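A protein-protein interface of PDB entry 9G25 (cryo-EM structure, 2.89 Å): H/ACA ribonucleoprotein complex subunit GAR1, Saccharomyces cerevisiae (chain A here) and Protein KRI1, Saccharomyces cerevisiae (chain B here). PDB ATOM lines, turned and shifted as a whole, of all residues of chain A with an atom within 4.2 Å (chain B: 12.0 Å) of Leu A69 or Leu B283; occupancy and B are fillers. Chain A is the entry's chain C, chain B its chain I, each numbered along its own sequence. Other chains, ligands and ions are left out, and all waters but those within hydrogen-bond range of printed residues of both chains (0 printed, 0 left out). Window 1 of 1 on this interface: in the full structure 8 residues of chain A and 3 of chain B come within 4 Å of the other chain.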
ATOM      1  N   TYR A  68      13.984 -14.158   2.280  1.00  0.00           N
ATOM      2  CA  TYR A  68      14.970 -15.112   2.754  1.00  0.00           C
ATOM      3  C   TYR A  68      16.302 -14.418   3.000  1.00  0.00           C
ATOM      4  O   TYR A  68      16.454 -13.215   2.781  1.00  0.00           O
ATOM      5  CB  TYR A  68      15.157 -16.242   1.732  1.00  0.00           C
ATOM      6  CG  TYR A  68      13.907 -17.049   1.480  1.00  0.00           C
ATOM      7  CD1 TYR A  68      13.009 -17.306   2.500  1.00  0.00           C
ATOM      8  CD2 TYR A  68      13.592 -17.495   0.208  1.00  0.00           C
ATOM      9  CE1 TYR A  68      11.858 -18.027   2.272  1.00  0.00           C
ATOM     10  CE2 TYR A  68      12.440 -18.208  -0.031  1.00  0.00           C
ATOM     11  CZ  TYR A  68      11.577 -18.473   1.005  1.00  0.00           C
ATOM     12  OH  TYR A  68      10.427 -19.187   0.775  1.00  0.00           O
ATOM     13  N   LEU A  69      17.265 -15.203   3.472  1.00  0.00           N
ATOM     14  CA  LEU A  69      18.661 -14.806   3.527  1.00  0.00           C
ATOM     15  C   LEU A  69      19.481 -15.658   2.559  1.00  0.00           C
ATOM     16  O   LEU A  69      18.944 -16.421   1.752  1.00  0.00           O
ATOM     17  CB  LEU A  69      19.207 -14.943   4.946  1.00  0.00           C
ATOM     18  CG  LEU A  69      18.554 -14.100   6.038  1.00  0.00           C
ATOM     19  CD1 LEU A  69      19.322 -14.237   7.337  1.00  0.00           C
ATOM     20  CD2 LEU A  69      18.468 -12.647   5.618  1.00  0.00           C
ATOM     21  N   GLU A  70      20.806 -15.514   2.638  1.00  0.00           N
ATOM     22  CA  GLU A  70      21.685 -16.403   1.883  1.00  0.00           C
ATOM     23  C   GLU A  70      21.673 -17.815   2.457  1.00  0.00           C
ATOM     24  O   GLU A  70      22.093 -18.768   1.793  1.00  0.00           O
ATOM     25  CB  GLU A  70      23.112 -15.855   1.866  1.00  0.00           C
ATOM     26  CG  GLU A  70      23.279 -14.570   1.097  1.00  0.00           C
ATOM     27  CD  GLU A  70      24.702 -14.058   1.124  1.00  0.00           C
ATOM     28  OE1 GLU A  70      25.530 -14.644   1.850  1.00  0.00           O
ATOM     29  OE2 GLU A  70      24.993 -13.068   0.421  1.00  0.00           O
ATOM     30  N   ASN A  71      21.202 -17.966   3.694  1.00  0.00           N
ATOM     31  CA  ASN A  71      21.133 -19.262   4.354  1.00  0.00           C
ATOM     32  C   ASN A  71      19.826 -19.970   4.028  1.00  0.00           C
ATOM     33  O   ASN A  71      19.534 -21.027   4.595  1.00  0.00           O
ATOM     34  CB  ASN A  71      21.274 -19.090   5.866  1.00  0.00           C
ATOM     35  CG  ASN A  71      22.562 -18.405   6.253  1.00  0.00           C
ATOM     36  OD1 ASN A  71      22.558 -17.264   6.712  1.00  0.00           O
ATOM     37  ND2 ASN A  71      23.680 -19.097   6.065  1.00  0.00           N
ATOM     38  N   LYS A  72      19.027 -19.364   3.147  1.00  0.00           N
ATOM     39  CA  LYS A  72      17.703 -19.799   2.681  1.00  0.00           C
ATOM     40  C   LYS A  72      16.671 -19.769   3.802  1.00  0.00           C
ATOM     41  O   LYS A  72      15.587 -20.347   3.643  1.00  0.00           O
ATOM     42  CB  LYS A  72      17.705 -21.199   2.053  1.00  0.00           C
ATOM     43  CG  LYS A  72      18.640 -21.406   0.859  1.00  0.00           C
ATOM     44  CD  LYS A  72      18.796 -20.175  -0.019  1.00  0.00           C
ATOM     45  CE  LYS A  72      19.717 -20.465  -1.197  1.00  0.00           C
ATOM     46  NZ  LYS A  72      20.676 -19.347  -1.444  1.00  0.00           N
ATOM     47  N   THR A  73      16.967 -19.118   4.924  1.00  0.00           N
ATOM     48  CA  THR A  73      16.045 -19.082   6.052  1.00  0.00           C
ATOM     49  C   THR A  73      15.129 -17.872   5.941  1.00  0.00           C
ATOM     50  O   THR A  73      15.584 -16.763   5.639  1.00  0.00           O
ATOM     51  CB  THR A  73      16.823 -19.047   7.364  1.00  0.00           C
ATOM     52  OG1 THR A  73      17.824 -18.027   7.297  1.00  0.00           O
ATOM     53  CG2 THR A  73      17.486 -20.388   7.625  1.00  0.00           C
ATOM     54  N   VAL A  75      12.948 -14.770   6.919  1.00  0.00           N
ATOM     55  CA  VAL A  75      12.835 -13.745   7.940  1.00  0.00           C
ATOM     56  C   VAL A  75      11.452 -13.105   7.963  1.00  0.00           C
ATOM     57  O   VAL A  75      11.111 -12.432   8.943  1.00  0.00           O
ATOM     58  CB  VAL A  75      13.924 -12.666   7.764  1.00  0.00           C
ATOM     59  CG1 VAL A  75      15.276 -13.308   7.609  1.00  0.00           C
ATOM     60  CG2 VAL A  75      13.619 -11.778   6.575  1.00  0.00           C
ATOM     61  N   VAL A  98      11.820 -12.596  14.657  1.00  0.00           N
ATOM     62  CA  VAL A  98      12.598 -11.753  13.759  1.00  0.00           C
ATOM     63  C   VAL A  98      12.317 -10.305  14.126  1.00  0.00           C
ATOM     64  O   VAL A  98      11.171  -9.849  14.051  1.00  0.00           O
ATOM     65  CB  VAL A  98      12.250 -12.027  12.288  1.00  0.00           C
ATOM     66  CG1 VAL A  98      13.169 -11.240  11.370  1.00  0.00           C
ATOM     67  CG2 VAL A  98      12.332 -13.515  11.993  1.00  0.00           C
ATOM     68  N   LYS A 108      21.371  -7.764   3.019  1.00  0.00           N
ATOM     69  CA  LYS A 108      20.635  -8.105   1.814  1.00  0.00           C
ATOM     70  C   LYS A 108      19.548  -9.119   2.135  1.00  0.00           C
ATOM     71  O   LYS A 108      19.740 -10.033   2.940  1.00  0.00           O
ATOM     72  CB  LYS A 108      21.565  -8.658   0.733  1.00  0.00           C
ATOM     73  CG  LYS A 108      22.531  -7.630   0.177  1.00  0.00           C
ATOM     74  CD  LYS A 108      23.405  -8.223  -0.904  1.00  0.00           C
ATOM     75  CE  LYS A 108      24.383  -7.194  -1.435  1.00  0.00           C
ATOM     76  NZ  LYS A 108      25.263  -7.758  -2.494  1.00  0.00           N
ATOM     77  N   PHE A 109      18.397  -8.940   1.496  1.00  0.00           N
ATOM     78  CA  PHE A 109      17.238  -9.797   1.680  1.00  0.00           C
ATOM     79  C   PHE A 109      16.857 -10.383   0.331  1.00  0.00           C
ATOM     80  O   PHE A 109      16.821  -9.663  -0.672  1.00  0.00           O
ATOM     81  CB  PHE A 109      16.071  -9.018   2.281  1.00  0.00           C
ATOM     82  CG  PHE A 109      16.365  -8.446   3.632  1.00  0.00           C
ATOM     83  CD1 PHE A 109      16.304  -9.236   4.763  1.00  0.00           C
ATOM     84  CD2 PHE A 109      16.720  -7.119   3.768  1.00  0.00           C
ATOM     85  CE1 PHE A 109      16.577  -8.707   6.003  1.00  0.00           C
ATOM     86  CE2 PHE A 109      16.993  -6.586   5.005  1.00  0.00           C
ATOM     87  CZ  PHE A 109      16.925  -7.379   6.122  1.00  0.00           C
ATOM     88  N   TYR A 110      16.549 -11.676   0.325  1.00  0.00           N
ATOM     89  CA  TYR A 110      16.476 -12.479  -0.886  1.00  0.00           C
ATOM     90  C   TYR A 110      15.056 -12.973  -1.119  1.00  0.00           C
ATOM     91  O   TYR A 110      14.306 -13.216  -0.170  1.00  0.00           O
ATOM     92  CB  TYR A 110      17.441 -13.667  -0.801  1.00  0.00           C
ATOM     93  CG  TYR A 110      18.895 -13.279  -0.939  1.00  0.00           C
ATOM     94  CD1 TYR A 110      19.552 -12.592   0.071  1.00  0.00           C
ATOM     95  CD2 TYR A 110      19.613 -13.619  -2.071  1.00  0.00           C
ATOM     96  CE1 TYR A 110      20.869 -12.228  -0.055  1.00  0.00           C
ATOM     97  CE2 TYR A 110      20.935 -13.264  -2.206  1.00  0.00           C
ATOM     98  CZ  TYR A 110      21.559 -12.569  -1.195  1.00  0.00           C
ATOM     99  OH  TYR A 110      22.880 -12.216  -1.316  1.00  0.00           O
ATOM    100  N   ARG B 278      26.293 -30.776  14.882  1.00  0.00           N
ATOM    101  CA  ARG B 278      26.935 -29.520  15.256  1.00  0.00           C
ATOM    102  C   ARG B 278      26.485 -28.372  14.360  1.00  0.00           C
ATOM    103  O   ARG B 278      26.479 -27.210  14.784  1.00  0.00           O
ATOM    104  CB  ARG B 278      28.455 -29.677  15.212  1.00  0.00           C
ATOM    105  CG  ARG B 278      29.005 -30.634  16.255  1.00  0.00           C
ATOM    106  CD  ARG B 278      29.051 -29.989  17.623  1.00  0.00           C
ATOM    107  NE  ARG B 278      30.203 -29.113  17.791  1.00  0.00           N
ATOM    108  CZ  ARG B 278      31.256 -29.397  18.545  1.00  0.00           C
ATOM    109  NH1 ARG B 278      31.323 -30.518  19.242  1.00  0.00           N
ATOM    110  NH2 ARG B 278      32.260 -28.528  18.611  1.00  0.00           N
ATOM    111  N   SER B 279      26.104 -28.671  13.121  1.00  0.00           N
ATOM    112  CA  SER B 279      25.739 -27.649  12.148  1.00  0.00           C
ATOM    113  C   SER B 279      24.244 -27.714  11.865  1.00  0.00           C
ATOM    114  O   SER B 279      23.721 -28.774  11.504  1.00  0.00           O
ATOM    115  CB  SER B 279      26.532 -27.826  10.855  1.00  0.00           C
ATOM    116  OG  SER B 279      26.181 -29.035  10.206  1.00  0.00           O
ATOM    117  N   GLN B 280      23.562 -26.580  12.025  1.00  0.00           N
ATOM    118  CA  GLN B 280      22.156 -26.438  11.668  1.00  0.00           C
ATOM    119  C   GLN B 280      21.988 -25.194  10.812  1.00  0.00           C
ATOM    120  O   GLN B 280      22.680 -24.193  11.027  1.00  0.00           O
ATOM    121  CB  GLN B 280      21.256 -26.329  12.906  1.00  0.00           C
ATOM    122  CG  GLN B 280      21.133 -27.596  13.729  1.00  0.00           C
ATOM    123  CD  GLN B 280      22.121 -27.645  14.874  1.00  0.00           C
ATOM    124  OE1 GLN B 280      22.727 -26.635  15.229  1.00  0.00           O
ATOM    125  NE2 GLN B 280      22.281 -28.821  15.463  1.00  0.00           N
ATOM    126  N   ALA B 281      21.077 -25.257   9.845  1.00  0.00           N
ATOM    127  CA  ALA B 281      20.704 -24.059   9.108  1.00  0.00           C
ATOM    128  C   ALA B 281      19.858 -23.159   9.997  1.00  0.00           C
ATOM    129  O   ALA B 281      18.726 -23.495  10.354  1.00  0.00           O
ATOM    130  CB  ALA B 281      19.939 -24.426   7.837  1.00  0.00           C
ATOM    131  N   THR B 282      20.414 -22.004  10.356  1.00  0.00           N
ATOM    132  CA  THR B 282      19.830 -21.171  11.395  1.00  0.00           C
ATOM    133  C   THR B 282      19.793 -19.720  10.942  1.00  0.00           C
ATOM    134  O   THR B 282      20.471 -19.320   9.993  1.00  0.00           O
ATOM    135  CB  THR B 282      20.613 -21.285  12.711  1.00  0.00           C
ATOM    136  OG1 THR B 282      19.964 -20.508  13.725  1.00  0.00           O
ATOM    137  CG2 THR B 282      22.033 -20.777  12.527  1.00  0.00           C
ATOM    138  N   LEU B 283      18.972 -18.936  11.639  1.00  0.00           N
ATOM    139  CA  LEU B 283      18.873 -17.506  11.389  1.00  0.00           C
ATOM    140  C   LEU B 283      19.924 -16.713  12.155  1.00  0.00           C
ATOM    141  O   LEU B 283      20.094 -15.517  11.896  1.00  0.00           O
ATOM    142  CB  LEU B 283      17.470 -17.021  11.763  1.00  0.00           C
ATOM    143  CG  LEU B 283      16.951 -15.731  11.135  1.00  0.00           C
ATOM    144  CD1 LEU B 283      16.850 -15.918   9.644  1.00  0.00           C
ATOM    145  CD2 LEU B 283      15.602 -15.356  11.718  1.00  0.00           C
ATOM    146  N   ARG B 284      20.636 -17.358  13.075  1.00  0.00           N
ATOM    147  CA  ARG B 284      21.566 -16.659  13.951  1.00  0.00           C
ATOM    148  C   ARG B 284      22.812 -16.220  13.193  1.00  0.00           C
ATOM    149  O   ARG B 284      23.347 -16.960  12.362  1.00  0.00           O
ATOM    150  CB  ARG B 284      21.953 -17.564  15.120  1.00  0.00           C
ATOM    151  CG  ARG B 284      22.730 -16.875  16.222  1.00  0.00           C
ATOM    152  CD  ARG B 284      22.980 -17.823  17.379  1.00  0.00           C
ATOM    153  NE  ARG B 284      21.811 -18.647  17.659  1.00  0.00           N
ATOM    154  CZ  ARG B 284      21.671 -19.411  18.733  1.00  0.00           C
ATOM    155  NH1 ARG B 284      22.611 -19.478  19.661  1.00  0.00           N
ATOM    156  NH2 ARG B 284      20.559 -20.124  18.880  1.00  0.00           N
ATOM    157  N   ARG B 285      23.270 -15.003  13.479  1.00  0.00           N
ATOM    158  CA  ARG B 285      24.504 -14.507  12.890  1.00  0.00           C
ATOM    159  C   ARG B 285      25.703 -15.269  13.443  1.00  0.00           C
ATOM    160  O   ARG B 285      25.782 -15.571  14.636  1.00  0.00           O
ATOM    161  CB  ARG B 285      24.675 -13.013  13.168  1.00  0.00           C
ATOM    162  CG  ARG B 285      23.659 -12.121  12.480  1.00  0.00           C
ATOM    163  CD  ARG B 285      23.926 -10.652  12.785  1.00  0.00           C
ATOM    164  NE  ARG B 285      22.913  -9.773  12.212  1.00  0.00           N
ATOM    165  CZ  ARG B 285      22.970  -9.256  10.993  1.00  0.00           C
ATOM    166  NH1 ARG B 285      23.974  -9.522  10.175  1.00  0.00           N
ATOM    167  NH2 ARG B 285      21.991  -8.454  10.582  1.00  0.00           N
ATOM    168  N   SER B 286      26.647 -15.577  12.557  1.00  0.00           N
ATOM    169  CA  SER B 286      27.847 -16.319  12.921  1.00  0.00           C
ATOM    170  C   SER B 286      29.063 -15.462  12.614  1.00  0.00           C
ATOM    171  O   SER B 286      29.361 -15.202  11.444  1.00  0.00           O
ATOM    172  CB  SER B 286      27.921 -17.651  12.168  1.00  0.00           C
ATOM    173  OG  SER B 286      27.898 -17.446  10.766  1.00  0.00           O
ATOM    174  N   ASP B 287      29.758 -15.024  13.659  1.00  0.00           N
ATOM    175  CA  ASP B 287      30.969 -14.239  13.468  1.00  0.00           C
ATOM    176  C   ASP B 287      32.125 -15.110  12.982  1.00  0.00           C
ATOM    177  O   ASP B 287      32.209 -16.300  13.294  1.00  0.00           O
ATOM    178  CB  ASP B 287      31.330 -13.488  14.758  1.00  0.00           C
ATOM    179  CG  ASP B 287      31.658 -14.408  15.934  1.00  0.00           C
ATOM    180  OD1 ASP B 287      31.417 -15.631  15.870  1.00  0.00           O
ATOM    181  OD2 ASP B 287      32.169 -13.887  16.948  1.00  0.00           O
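The backbone NH (N) of Arg B284 is in hydrogen-bond range of the side-chain hydroxyl (OG1) of Thr B282 (3.3 Å).
Of the 11 printed residues of chain A, 4 touch a printed residue of chain B. Printed residues of chain A that touch a printed residue of chain B: Leu A69, Thr A73, Val A75 and Val A98. Hydrophobic or aromatic side chains of chain A that line the printed part of chain B: Leu A69, Val A75 and Val A98. Along chain A the printed residues that touch a printed residue of chain B span positions 69 to 98. Of the 10 printed residues of chain B, 2 touch a printed residue of chain A. Hydrophobic or aromatic side chains of chain B that line the printed part of chain A: Leu B283. Among the printed residues, 5 pairs touch across the chains. Among the printed residues, no Asp or Glu carboxylate lies within 4 Å of a Lys or Arg side-chain nitrogen of the other chain.
Among the printed residues, merely in contact across the chains: Leu A69 with Leu B283 (3.8 Å), Thr A73 with Thr B282 (3.96 Å), Thr A73 with Leu B283 (3.3 Å), Val A75 with Leu B283 (3.7 Å) and Val A98 with Leu B283 (3.8 Å).
Leu A69 touches just one residue of chain B: Leu B283 (3.8 Å). No residue of chain B comes within 4 Å of Glu A70. No residue of chain B comes within 4 Å of Asn A71. No residue of chain B comes within 4 Å of Lys A72. Thr A73 touches two residues of chain B. Of chain B, only Leu B283 (3.7 Å) comes within 4 Å of Val A75. No residue of chain B comes within 4 Å of Tyr A110. Printed residues of chain A within 4 Å of Thr B282: Thr A73. Leu B283 touches four residues of chain A.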
